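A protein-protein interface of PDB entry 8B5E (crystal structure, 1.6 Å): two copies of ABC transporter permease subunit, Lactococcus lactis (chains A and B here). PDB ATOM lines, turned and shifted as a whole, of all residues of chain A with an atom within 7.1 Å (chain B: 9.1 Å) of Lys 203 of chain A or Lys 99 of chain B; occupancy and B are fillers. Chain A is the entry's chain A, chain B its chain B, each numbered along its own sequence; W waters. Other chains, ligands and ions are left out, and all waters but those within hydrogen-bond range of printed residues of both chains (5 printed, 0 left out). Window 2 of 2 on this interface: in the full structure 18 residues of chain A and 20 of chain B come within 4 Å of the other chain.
The side-chain amide nitrogen (ND2) of Asn 83 of chain A sits at hydrogen-bond distance from the backbone carbonyl oxygen (O) of Asn 175 of chain B, at 3.3 Å. The side-chain amide nitrogen (ND2) of Asn 83 of chain A sits at hydrogen-bond distance from the backbone carbonyl oxygen (O) of Ser 101 of chain B, 2.9 Å away.
ND2 of Asn 175 of chain B is in hydrogen-bond range of O of Leu 100 of chain B, at 2.9 Å. N of Ser 101 of chain B is in hydrogen-bond range of OD2 of Asp 105 of chain B (3.0 Å). The backbone carbonyl oxygen (O) of Ser 98 of chain B lies within hydrogen-bond range of the side-chain amide nitrogen (ND2) of Asn 175 of chain B. The side-chain amide oxygen (OD1) of Asn 202 of chain A lies within hydrogen-bond range of the backbone NH (N) of Asn 83 of chain A. NZ of Lys 203 of chain A lies within salt-bridge range of OD1 of Asp 199 of chain A, at 3.1 Å.
Among the printed residues, merely in contact across the chains: Asn 202 of chain A with Ser 101 of chain B, Lys 203 of chain A with Lys 99 of chain B, Ala 206 of chain A with Met 174 of chain B, Ala 206 of chain A with Asn 175 of chain B, Lys 209 of chain A with Met 174 of chain B and Lys 209 of chain A with Phe 176 of chain B.
No residue of chain B comes within 4 Å of Gly 200 of chain A. Of the printed residues of chain B, Lys 203 of chain A touches Lys 99 (3.5 Å). Ala 204 of chain A touches none of the printed residues of chain B. Of the printed residues of chain B, Ala 206 of chain A touches Met 174 (3.3 Å) and Asn 175 (3.5 Å). Lys 99 of chain B touches just one residue of chain A: Lys 203. Of the printed residues of chain A, Ser 101 of chain B touches Asn 83 (2.9 Å) and Asn 202 (3.8 Å). Printed residues of chain A within 4 Å of Met 174 of chain B: Ala 206 and Lys 209. Of the printed residues of chain A, Asn 175 of chain B touches Asn 83 (3.3 Å) and Ala 206 (3.5 Å). Printed residues of chain A within 4 Å of Phe 176 of chain B: Lys 209. The nearest printed residue of chain A that does not touch Asn 175 of chain B is Asn 202 of chain A (5.0 Å).
Hydrophobic or aromatic side chains of chain B that line the printed part of chain A: Met 174. Along chain B the printed residues that touch a printed residue of chain A span positions 99 to 176. Of the 17 printed residues of chain A, 5 touch a printed residue of chain B. Among the printed residues, 8 pairs touch across the chains. Among the printed residues, no Asp or Glu carboxylate lies within 4 Å of a Lys or Arg side-chain nitrogen of the other chain.
No position is printed for both chains. Of the 8 pairs that touch across the chains among the printed residues, none has its exchanged pair printed and touching as well.
Water W5 lies within hydrogen-bond range of OD1 of Asn 83 of chain A (2.4 Å) and OD2 of Asp 102 of chain B (3.1 Å). Water W3 lies within hydrogen-bond range of OG of Ser 101 of chain B (2.5 Å), OD1 of Asp 199 of chain A (2.7 Å) and ND2 of Asn 202 of chain A (3.1 Å). Water W2 lies within hydrogen-bond range of O of Asn 175 of chain B (2.8 Å) and O of Asn 202 of chain A (3.0 Å). Water W4 lies within hydrogen-bond range of the backbone carbonyl oxygen (O) of Asn 202 of chain A (2.9 Å), the side-chain amide nitrogen (ND2) of Asn 83 of chain A (3.0 Å) and the backbone carbonyl oxygen (O) of Asn 175 of chain B (3.3 Å). Water W1 lies within hydrogen-bond range of the backbone carbonyl oxygen (O) of Met 174 of chain B (2.9 Å), the backbone carbonyl oxygen (O) of Phe 176 of chain B (3.0 Å) and the side-chain amino group (NZ) of Lys 209 of chain A (3.3 Å).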
ATOM      1  N   VAL A  35     -19.741  10.892 -19.037  1.00  0.00           N
ATOM      2  CA  VAL A  35     -18.353  11.074 -19.470  1.00  0.00           C
ATOM      3  C   VAL A  35     -17.495  11.536 -18.277  1.00  0.00           C
ATOM      4  O   VAL A  35     -16.359  11.091 -18.084  1.00  0.00           O
ATOM      5  CB  VAL A  35     -18.289  12.069 -20.652  1.00  0.00           C
ATOM      6  CG1 VAL A  35     -16.882  12.577 -20.924  1.00  0.00           C
ATOM      7  CG2 VAL A  35     -18.893  11.453 -21.904  1.00  0.00           C
ATOM      8  N   ILE A  38     -16.919   8.655 -15.771  1.00  0.00           N
ATOM      9  CA  ILE A  38     -15.953   7.712 -16.344  1.00  0.00           C
ATOM     10  C   ILE A  38     -14.521   8.250 -16.230  1.00  0.00           C
ATOM     11  O   ILE A  38     -13.605   7.469 -15.956  1.00  0.00           O
ATOM     12  CB  ILE A  38     -16.320   7.278 -17.781  1.00  0.00           C
ATOM     13  CG1 ILE A  38     -17.571   6.404 -17.762  1.00  0.00           C
ATOM     14  CG2 ILE A  38     -15.163   6.533 -18.467  1.00  0.00           C
ATOM     15  CD1 ILE A  38     -18.249   6.233 -19.081  1.00  0.00           C
ATOM     16  N   ASN A  39     -14.326   9.560 -16.415  1.00  0.00           N
ATOM     17  CA  ASN A  39     -13.018  10.172 -16.464  1.00  0.00           C
ATOM     18  C   ASN A  39     -12.551  10.739 -15.119  1.00  0.00           C
ATOM     19  O   ASN A  39     -11.446  11.271 -15.046  1.00  0.00           O
ATOM     20  CB  ASN A  39     -12.980  11.233 -17.563  1.00  0.00           C
ATOM     21  CG  ASN A  39     -12.888  10.619 -18.953  1.00  0.00           C
ATOM     22  OD1 ASN A  39     -11.831  10.153 -19.354  1.00  0.00           O
ATOM     23  ND2 ASN A  39     -13.978  10.591 -19.690  1.00  0.00           N
ATOM     24  N   ASN A  83     -15.365  12.829 -31.656  1.00  0.00           N
ATOM     25  CA  ASN A  83     -16.171  12.032 -32.555  1.00  0.00           C
ATOM     26  C   ASN A  83     -17.616  12.450 -32.339  1.00  0.00           C
ATOM     27  O   ASN A  83     -18.007  12.784 -31.225  1.00  0.00           O
ATOM     28  CB  ASN A  83     -16.064  10.532 -32.304  1.00  0.00           C
ATOM     29  CG  ASN A  83     -14.707   9.957 -32.681  1.00  0.00           C
ATOM     30  OD1 ASN A  83     -14.041  10.485 -33.568  1.00  0.00           O
ATOM     31  ND2 ASN A  83     -14.307   8.875 -32.020  1.00  0.00           N
ATOM     32  N   LEU A 197      -9.757  16.630 -22.764  1.00  0.00           N
ATOM     33  CA  LEU A 197     -11.201  16.577 -22.660  1.00  0.00           C
ATOM     34  C   LEU A 197     -11.780  15.867 -23.881  1.00  0.00           C
ATOM     35  O   LEU A 197     -12.666  15.049 -23.748  1.00  0.00           O
ATOM     36  CB  LEU A 197     -11.747  18.009 -22.518  1.00  0.00           C
ATOM     37  CG  LEU A 197     -11.258  18.801 -21.311  1.00  0.00           C
ATOM     38  CD1 LEU A 197     -12.029  20.088 -21.213  1.00  0.00           C
ATOM     39  CD2 LEU A 197     -11.466  18.001 -20.036  1.00  0.00           C
ATOM     40  N   VAL A 198     -11.261  16.167 -25.080  1.00  0.00           N
ATOM     41  CA  VAL A 198     -11.728  15.525 -26.297  1.00  0.00           C
ATOM     42  C   VAL A 198     -11.447  14.017 -26.251  1.00  0.00           C
ATOM     43  O   VAL A 198     -12.316  13.206 -26.592  1.00  0.00           O
ATOM     44  CB  VAL A 198     -11.133  16.198 -27.549  1.00  0.00           C
ATOM     45  CG1 VAL A 198     -11.503  15.442 -28.814  1.00  0.00           C
ATOM     46  CG2 VAL A 198     -11.528  17.667 -27.674  1.00  0.00           C
ATOM     47  N   ASP A 199     -10.234  13.641 -25.791  1.00  0.00           N
ATOM     48  CA  ASP A 199      -9.874  12.232 -25.727  1.00  0.00           C
ATOM     49  C   ASP A 199     -10.734  11.504 -24.698  1.00  0.00           C
ATOM     50  O   ASP A 199     -11.235  10.409 -24.970  1.00  0.00           O
ATOM     51  CB  ASP A 199      -8.386  12.046 -25.404  1.00  0.00           C
ATOM     52  CG  ASP A 199      -7.920  10.599 -25.508  1.00  0.00           C
ATOM     53  OD1 ASP A 199      -8.211   9.941 -26.540  1.00  0.00           O
ATOM     54  OD2 ASP A 199      -7.244  10.133 -24.561  1.00  0.00           O
ATOM     55  N   GLY A 200     -10.949  12.134 -23.534  1.00  0.00           N
ATOM     56  CA  GLY A 200     -11.802  11.550 -22.509  1.00  0.00           C
ATOM     57  C   GLY A 200     -13.233  11.346 -23.009  1.00  0.00           C
ATOM     58  O   GLY A 200     -13.868  10.309 -22.777  1.00  0.00           O
ATOM     59  N   PHE A 201     -13.723  12.336 -23.783  1.00  0.00           N
ATOM     60  CA  PHE A 201     -15.054  12.234 -24.358  1.00  0.00           C
ATOM     61  C   PHE A 201     -15.117  11.040 -25.315  1.00  0.00           C
ATOM     62  O   PHE A 201     -16.025  10.217 -25.232  1.00  0.00           O
ATOM     63  CB  PHE A 201     -15.498  13.584 -24.943  1.00  0.00           C
ATOM     64  CG  PHE A 201     -16.950  13.633 -25.309  1.00  0.00           C
ATOM     65  CD1 PHE A 201     -17.403  13.037 -26.482  1.00  0.00           C
ATOM     66  CD2 PHE A 201     -17.880  14.245 -24.467  1.00  0.00           C
ATOM     67  CE1 PHE A 201     -18.751  13.038 -26.806  1.00  0.00           C
ATOM     68  CE2 PHE A 201     -19.226  14.258 -24.801  1.00  0.00           C
ATOM     69  CZ  PHE A 201     -19.651  13.674 -25.973  1.00  0.00           C
ATOM     70  N   ASN A 202     -14.143  10.950 -26.213  1.00  0.00           N
ATOM     71  CA  ASN A 202     -14.099   9.874 -27.231  1.00  0.00           C
ATOM     72  C   ASN A 202     -14.063   8.499 -26.566  1.00  0.00           C
ATOM     73  O   ASN A 202     -14.794   7.621 -26.992  1.00  0.00           O
ATOM     74  CB  ASN A 202     -12.889  10.046 -28.152  1.00  0.00           C
ATOM     75  CG  ASN A 202     -13.093  11.170 -29.132  1.00  0.00           C
ATOM     76  OD1 ASN A 202     -14.204  11.665 -29.234  1.00  0.00           O
ATOM     77  ND2 ASN A 202     -12.043  11.584 -29.817  1.00  0.00           N
ATOM     78  N   LYS A 203     -13.221   8.343 -25.557  1.00  0.00           N
ATOM     79  CA  LYS A 203     -13.046   7.008 -24.926  1.00  0.00           C
ATOM     80  C   LYS A 203     -14.293   6.665 -24.097  1.00  0.00           C
ATOM     81  O   LYS A 203     -14.713   5.530 -24.143  1.00  0.00           O
ATOM     82  CB  LYS A 203     -11.748   7.006 -24.117  1.00  0.00           C
ATOM     83  CG  LYS A 203     -10.491   6.871 -24.957  1.00  0.00           C
ATOM     84  CD  LYS A 203      -9.259   7.412 -24.289  1.00  0.00           C
ATOM     85  CE  LYS A 203      -7.978   6.921 -24.929  1.00  0.00           C
ATOM     86  NZ  LYS A 203      -8.086   6.877 -26.406  1.00  0.00           N
ATOM     87  N   ALA A 204     -14.839   7.639 -23.367  1.00  0.00           N
ATOM     88  CA  ALA A 204     -16.051   7.393 -22.572  1.00  0.00           C
ATOM     89  C   ALA A 204     -17.261   7.070 -23.449  1.00  0.00           C
ATOM     90  O   ALA A 204     -18.024   6.145 -23.156  1.00  0.00           O
ATOM     91  CB  ALA A 204     -16.342   8.578 -21.681  1.00  0.00           C
ATOM     92  N   LEU A 205     -17.415   7.793 -24.570  1.00  0.00           N
ATOM     93  CA  LEU A 205     -18.485   7.492 -25.500  1.00  0.00           C
ATOM     94  C   LEU A 205     -18.393   6.058 -26.010  1.00  0.00           C
ATOM     95  O   LEU A 205     -19.416   5.368 -26.150  1.00  0.00           O
ATOM     96  CB  LEU A 205     -18.430   8.456 -26.690  1.00  0.00           C
ATOM     97  CG  LEU A 205     -19.567   8.287 -27.689  1.00  0.00           C
ATOM     98  CD1 LEU A 205     -20.895   8.757 -27.039  1.00  0.00           C
ATOM     99  CD2 LEU A 205     -19.233   9.033 -29.001  1.00  0.00           C
ATOM    100  N   ALA A 206     -17.170   5.633 -26.356  1.00  0.00           N
ATOM    101  CA  ALA A 206     -16.957   4.275 -26.832  1.00  0.00           C
ATOM    102  C   ALA A 206     -17.379   3.264 -25.764  1.00  0.00           C
ATOM    103  O   ALA A 206     -18.057   2.281 -26.092  1.00  0.00           O
ATOM    104  CB  ALA A 206     -15.524   4.121 -27.221  1.00  0.00           C
ATOM    105  N   GLU A 207     -17.028   3.519 -24.490  1.00  0.00           N
ATOM    106  CA  GLU A 207     -17.430   2.607 -23.419  1.00  0.00           C
ATOM    107  C   GLU A 207     -18.953   2.579 -23.275  1.00  0.00           C
ATOM    108  O   GLU A 207     -19.544   1.500 -23.156  1.00  0.00           O
ATOM    109  CB  GLU A 207     -16.827   2.930 -22.048  1.00  0.00           C
ATOM    110  CG  GLU A 207     -17.404   2.062 -20.911  1.00  0.00           C
ATOM    111  CD  GLU A 207     -16.995   0.590 -20.842  1.00  0.00           C
ATOM    112  OE1 GLU A 207     -16.125   0.184 -21.630  1.00  0.00           O
ATOM    113  OE2 GLU A 207     -17.554  -0.162 -19.978  1.00  0.00           O
ATOM    114  N   MET A 208     -19.577   3.767 -23.283  1.00  0.00           N
ATOM    115  CA  MET A 208     -21.027   3.886 -23.152  1.00  0.00           C
ATOM    116  C   MET A 208     -21.764   3.259 -24.353  1.00  0.00           C
ATOM    117  O   MET A 208     -22.829   2.643 -24.184  1.00  0.00           O
ATOM    118  CB  MET A 208     -21.415   5.360 -23.056  1.00  0.00           C
ATOM    119  CG  MET A 208     -20.962   6.014 -21.800  1.00  0.00           C
ATOM    120  SD  MET A 208     -21.042   7.819 -21.859  1.00  0.00           S
ATOM    121  CE  MET A 208     -22.816   8.012 -22.049  1.00  0.00           C
ATOM    122  N   LYS A 209     -21.213   3.403 -25.582  1.00  0.00           N
ATOM    123  CA  LYS A 209     -21.822   2.720 -26.711  1.00  0.00           C
ATOM    124  C   LYS A 209     -21.677   1.204 -26.558  1.00  0.00           C
ATOM    125  O   LYS A 209     -22.570   0.453 -26.940  1.00  0.00           O
ATOM    126  CB  LYS A 209     -21.204   3.172 -28.039  1.00  0.00           C
ATOM    127  CG  LYS A 209     -21.684   4.509 -28.602  1.00  0.00           C
ATOM    128  CD  LYS A 209     -20.905   4.843 -29.858  1.00  0.00           C
ATOM    129  CE  LYS A 209     -21.373   6.013 -30.695  1.00  0.00           C
ATOM    130  NZ  LYS A 209     -20.557   6.094 -31.940  1.00  0.00           N
ATOM    131  N   THR B  94     -12.900  -2.116 -33.415  1.00  0.00           N
ATOM    132  CA  THR B  94     -11.551  -2.475 -32.989  1.00  0.00           C
ATOM    133  C   THR B  94     -11.636  -3.606 -31.966  1.00  0.00           C
ATOM    134  O   THR B  94     -12.723  -4.021 -31.564  1.00  0.00           O
ATOM    135  CB  THR B  94     -10.831  -1.277 -32.345  1.00  0.00           C
ATOM    136  OG1 THR B  94     -11.558  -0.845 -31.198  1.00  0.00           O
ATOM    137  CG2 THR B  94     -10.647  -0.104 -33.282  1.00  0.00           C
ATOM    138  N   THR B  95     -10.474  -4.101 -31.509  1.00  0.00           N
ATOM    139  CA  THR B  95     -10.480  -4.990 -30.359  1.00  0.00           C
ATOM    140  C   THR B  95     -10.820  -4.208 -29.091  1.00  0.00           C
ATOM    141  O   THR B  95     -10.732  -2.968 -29.075  1.00  0.00           O
ATOM    142  CB  THR B  95      -9.148  -5.742 -30.238  1.00  0.00           C
ATOM    143  OG1 THR B  95      -8.115  -4.764 -30.110  1.00  0.00           O
ATOM    144  CG2 THR B  95      -8.882  -6.645 -31.422  1.00  0.00           C
ATOM    145  N   LYS B  96     -11.128  -4.963 -28.024  1.00  0.00           N
ATOM    146  CA  LYS B  96     -11.720  -4.414 -26.811  1.00  0.00           C
ATOM    147  C   LYS B  96     -10.765  -3.439 -26.119  1.00  0.00           C
ATOM    148  O   LYS B  96     -11.234  -2.516 -25.459  1.00  0.00           O
ATOM    149  CB  LYS B  96     -12.179  -5.549 -25.880  1.00  0.00           C
ATOM    150  CG  LYS B  96     -11.099  -6.233 -25.038  1.00  0.00           C
ATOM    151  CD  LYS B  96     -11.644  -6.942 -23.805  1.00  0.00           C
ATOM    152  CE  LYS B  96     -10.663  -7.006 -22.649  1.00  0.00           C
ATOM    153  NZ  LYS B  96     -11.322  -7.482 -21.410  1.00  0.00           N
ATOM    154  N   ASP B  97      -9.438  -3.634 -26.267  1.00  0.00           N
ATOM    155  CA  ASP B  97      -8.435  -2.859 -25.534  1.00  0.00           C
ATOM    156  C   ASP B  97      -7.747  -1.833 -26.440  1.00  0.00           C
ATOM    157  O   ASP B  97      -6.816  -1.133 -26.036  1.00  0.00           O
ATOM    158  CB  ASP B  97      -7.415  -3.792 -24.867  1.00  0.00           C
ATOM    159  CG  ASP B  97      -7.968  -4.559 -23.675  1.00  0.00           C
ATOM    160  OD1 ASP B  97      -8.915  -4.053 -22.985  1.00  0.00           O
ATOM    161  OD2 ASP B  97      -7.444  -5.679 -23.430  1.00  0.00           O
ATOM    162  N   SER B  98      -8.220  -1.695 -27.681  1.00  0.00           N
ATOM    163  CA  SER B  98      -7.642  -0.738 -28.611  1.00  0.00           C
ATOM    164  C   SER B  98      -7.851   0.694 -28.120  1.00  0.00           C
ATOM    165  O   SER B  98      -8.932   1.028 -27.607  1.00  0.00           O
ATOM    166  CB  SER B  98      -8.247  -0.919 -29.966  1.00  0.00           C
ATOM    167  OG  SER B  98      -7.791   0.087 -30.840  1.00  0.00           O
ATOM    168  N   LYS B  99      -6.849   1.540 -28.333  1.00  0.00           N
ATOM    169  CA  LYS B  99      -6.986   2.963 -28.046  1.00  0.00           C
ATOM    170  C   LYS B  99      -7.154   3.801 -29.317  1.00  0.00           C
ATOM    171  O   LYS B  99      -7.100   5.024 -29.238  1.00  0.00           O
ATOM    172  CB  LYS B  99      -5.773   3.534 -27.311  1.00  0.00           C
ATOM    173  CG  LYS B  99      -5.390   2.801 -26.040  1.00  0.00           C
ATOM    174  CD  LYS B  99      -6.537   2.591 -25.079  1.00  0.00           C
ATOM    175  CE  LYS B  99      -6.262   1.451 -24.111  1.00  0.00           C
ATOM    176  NZ  LYS B  99      -5.442   1.962 -23.013  1.00  0.00           N
ATOM    177  N   LEU B 100      -7.359   3.174 -30.468  1.00  0.00           N
ATOM    178  CA  LEU B 100      -7.653   3.901 -31.698  1.00  0.00           C
ATOM    179  C   LEU B 100      -9.041   4.522 -31.561  1.00  0.00           C
ATOM    180  O   LEU B 100      -9.963   3.859 -31.074  1.00  0.00           O
ATOM    181  CB  LEU B 100      -7.618   2.926 -32.877  1.00  0.00           C
ATOM    182  CG  LEU B 100      -6.314   2.143 -33.042  1.00  0.00           C
ATOM    183  CD1 LEU B 100      -6.398   1.237 -34.252  1.00  0.00           C
ATOM    184  CD2 LEU B 100      -5.111   3.079 -33.136  1.00  0.00           C
ATOM    185  N   SER B 101      -9.185   5.798 -31.955  1.00  0.00           N
ATOM    186  CA  SER B 101     -10.466   6.475 -31.784  1.00  0.00           C
ATOM    187  C   SER B 101     -10.812   7.388 -32.963  1.00  0.00           C
ATOM    188  O   SER B 101     -11.998   7.647 -33.200  1.00  0.00           O
ATOM    189  CB  SER B 101     -10.553   7.164 -30.405  1.00  0.00           C
ATOM    190  OG  SER B 101      -9.950   8.437 -30.399  1.00  0.00           O
ATOM    191  N   ASP B 102      -9.796   7.804 -33.728  1.00  0.00           N
ATOM    192  CA  ASP B 102      -9.902   8.807 -34.780  1.00  0.00           C
ATOM    193  C   ASP B 102      -9.349   8.200 -36.072  1.00  0.00           C
ATOM    194  O   ASP B 102      -8.440   7.377 -36.030  1.00  0.00           O
ATOM    195  CB  ASP B 102      -9.119  10.050 -34.331  1.00  0.00           C
ATOM    196  CG  ASP B 102      -9.070  11.232 -35.292  1.00  0.00           C
ATOM    197  OD1 ASP B 102      -8.405  11.124 -36.370  1.00  0.00           O
ATOM    198  OD2 ASP B 102      -9.665  12.277 -34.950  1.00  0.00           O
ATOM    199  N   ASP B 105      -5.681   7.869 -36.733  1.00  0.00           N
ATOM    200  CA  ASP B 105      -4.987   6.840 -35.968  1.00  0.00           C
ATOM    201  C   ASP B 105      -4.762   5.573 -36.796  1.00  0.00           C
ATOM    202  O   ASP B 105      -3.976   4.733 -36.410  1.00  0.00           O
ATOM    203  CB  ASP B 105      -5.774   6.446 -34.707  1.00  0.00           C
ATOM    204  CG  ASP B 105      -5.928   7.528 -33.639  1.00  0.00           C
ATOM    205  OD1 ASP B 105      -5.143   8.492 -33.654  1.00  0.00           O
ATOM    206  OD2 ASP B 105      -6.847   7.405 -32.797  1.00  0.00           O
ATOM    207  N   LEU B 106      -5.421   5.457 -37.961  1.00  0.00           N
ATOM    208  CA  LEU B 106      -5.292   4.297 -38.826  1.00  0.00           C
ATOM    209  C   LEU B 106      -4.112   4.445 -39.775  1.00  0.00           C
ATOM    210  O   LEU B 106      -3.889   3.539 -40.572  1.00  0.00           O
ATOM    211  CB  LEU B 106      -6.586   4.108 -39.625  1.00  0.00           C
ATOM    212  CG  LEU B 106      -7.823   3.869 -38.764  1.00  0.00           C
ATOM    213  CD1 LEU B 106      -9.084   3.920 -39.611  1.00  0.00           C
ATOM    214  CD2 LEU B 106      -7.693   2.550 -37.995  1.00  0.00           C
ATOM    215  N   LYS B 109      -1.871   1.515 -40.984  1.00  0.00           N
ATOM    216  CA  LYS B 109      -2.524   0.326 -40.444  1.00  0.00           C
ATOM    217  C   LYS B 109      -3.400  -0.323 -41.514  1.00  0.00           C
ATOM    218  O   LYS B 109      -3.683   0.295 -42.529  1.00  0.00           O
ATOM    219  CB  LYS B 109      -3.241   0.701 -39.147  1.00  0.00           C
ATOM    220  CG  LYS B 109      -2.280   0.900 -37.982  1.00  0.00           C
ATOM    221  CD  LYS B 109      -2.900   1.460 -36.736  1.00  0.00           C
ATOM    222  CE  LYS B 109      -1.877   2.096 -35.821  1.00  0.00           C
ATOM    223  NZ  LYS B 109      -0.756   1.166 -35.522  1.00  0.00           N
ATOM    224  N   ALA B 153      -6.236  -3.543 -37.875  1.00  0.00           N
ATOM    225  CA  ALA B 153      -6.409  -2.629 -36.747  1.00  0.00           C
ATOM    226  C   ALA B 153      -7.890  -2.294 -36.508  1.00  0.00           C
ATOM    227  O   ALA B 153      -8.286  -1.911 -35.402  1.00  0.00           O
ATOM    228  CB  ALA B 153      -5.613  -1.366 -37.027  1.00  0.00           C
ATOM    229  N   ALA B 173     -14.753  -3.506 -29.589  1.00  0.00           N
ATOM    230  CA  ALA B 173     -15.264  -2.238 -29.085  1.00  0.00           C
ATOM    231  C   ALA B 173     -15.690  -1.328 -30.245  1.00  0.00           C
ATOM    232  O   ALA B 173     -15.211  -1.497 -31.378  1.00  0.00           O
ATOM    233  CB  ALA B 173     -14.213  -1.573 -28.230  1.00  0.00           C
ATOM    234  N   MET B 174     -16.554  -0.335 -29.924  1.00  0.00           N
ATOM    235  CA  MET B 174     -16.952   0.680 -30.895  1.00  0.00           C
ATOM    236  C   MET B 174     -16.332   2.022 -30.520  1.00  0.00           C
ATOM    237  O   MET B 174     -16.963   2.854 -29.874  1.00  0.00           O
ATOM    238  CB  MET B 174     -18.477   0.785 -30.960  1.00  0.00           C
ATOM    239  CG  MET B 174     -19.075  -0.342 -31.800  1.00  0.00           C
ATOM    240  SD  MET B 174     -20.889  -0.296 -31.934  1.00  0.00           S
ATOM    241  CE  MET B 174     -21.318  -0.571 -30.217  1.00  0.00           C
ATOM    242  N   ASN B 175     -15.095   2.221 -30.971  1.00  0.00           N
ATOM    243  CA  ASN B 175     -14.283   3.380 -30.644  1.00  0.00           C
ATOM    244  C   ASN B 175     -14.424   4.533 -31.655  1.00  0.00           C
ATOM    245  O   ASN B 175     -13.890   5.605 -31.429  1.00  0.00           O
ATOM    246  CB  ASN B 175     -12.796   2.998 -30.563  1.00  0.00           C
ATOM    247  CG  ASN B 175     -12.391   2.236 -29.317  1.00  0.00           C
ATOM    248  OD1 ASN B 175     -13.232   1.830 -28.535  1.00  0.00           O
ATOM    249  ND2 ASN B 175     -11.086   2.037 -29.125  1.00  0.00           N
ATOM    250  N   PHE B 176     -15.049   4.284 -32.806  1.00  0.00           N
ATOM    251  CA  PHE B 176     -15.067   5.234 -33.910  1.00  0.00           C
ATOM    252  C   PHE B 176     -16.470   5.814 -34.069  1.00  0.00           C
ATOM    253  O   PHE B 176     -17.469   5.282 -33.554  1.00  0.00           O
ATOM    254  CB  PHE B 176     -14.595   4.566 -35.198  1.00  0.00           C
ATOM    255  CG  PHE B 176     -13.102   4.430 -35.301  1.00  0.00           C
ATOM    256  CD1 PHE B 176     -12.442   3.404 -34.646  1.00  0.00           C
ATOM    257  CD2 PHE B 176     -12.346   5.297 -36.083  1.00  0.00           C
ATOM    258  CE1 PHE B 176     -11.056   3.289 -34.727  1.00  0.00           C
ATOM    259  CE2 PHE B 176     -10.964   5.169 -36.188  1.00  0.00           C
ATOM    260  CZ  PHE B 176     -10.324   4.165 -35.490  1.00  0.00           C
HETATM  261  O   HOH W   1     -17.567   5.616 -30.551  1.00  0.00           O
HETATM  262  O   HOH W   2     -12.911   6.148 -28.859  1.00  0.00           O
HETATM  263  O   HOH W   3      -9.374  10.357 -28.900  1.00  0.00           O
HETATM  264  O   HOH W   4     -15.753   7.679 -29.695  1.00  0.00           O
HETATM  265  O   HOH W   5     -12.708  12.419 -34.199  1.00  0.00           O
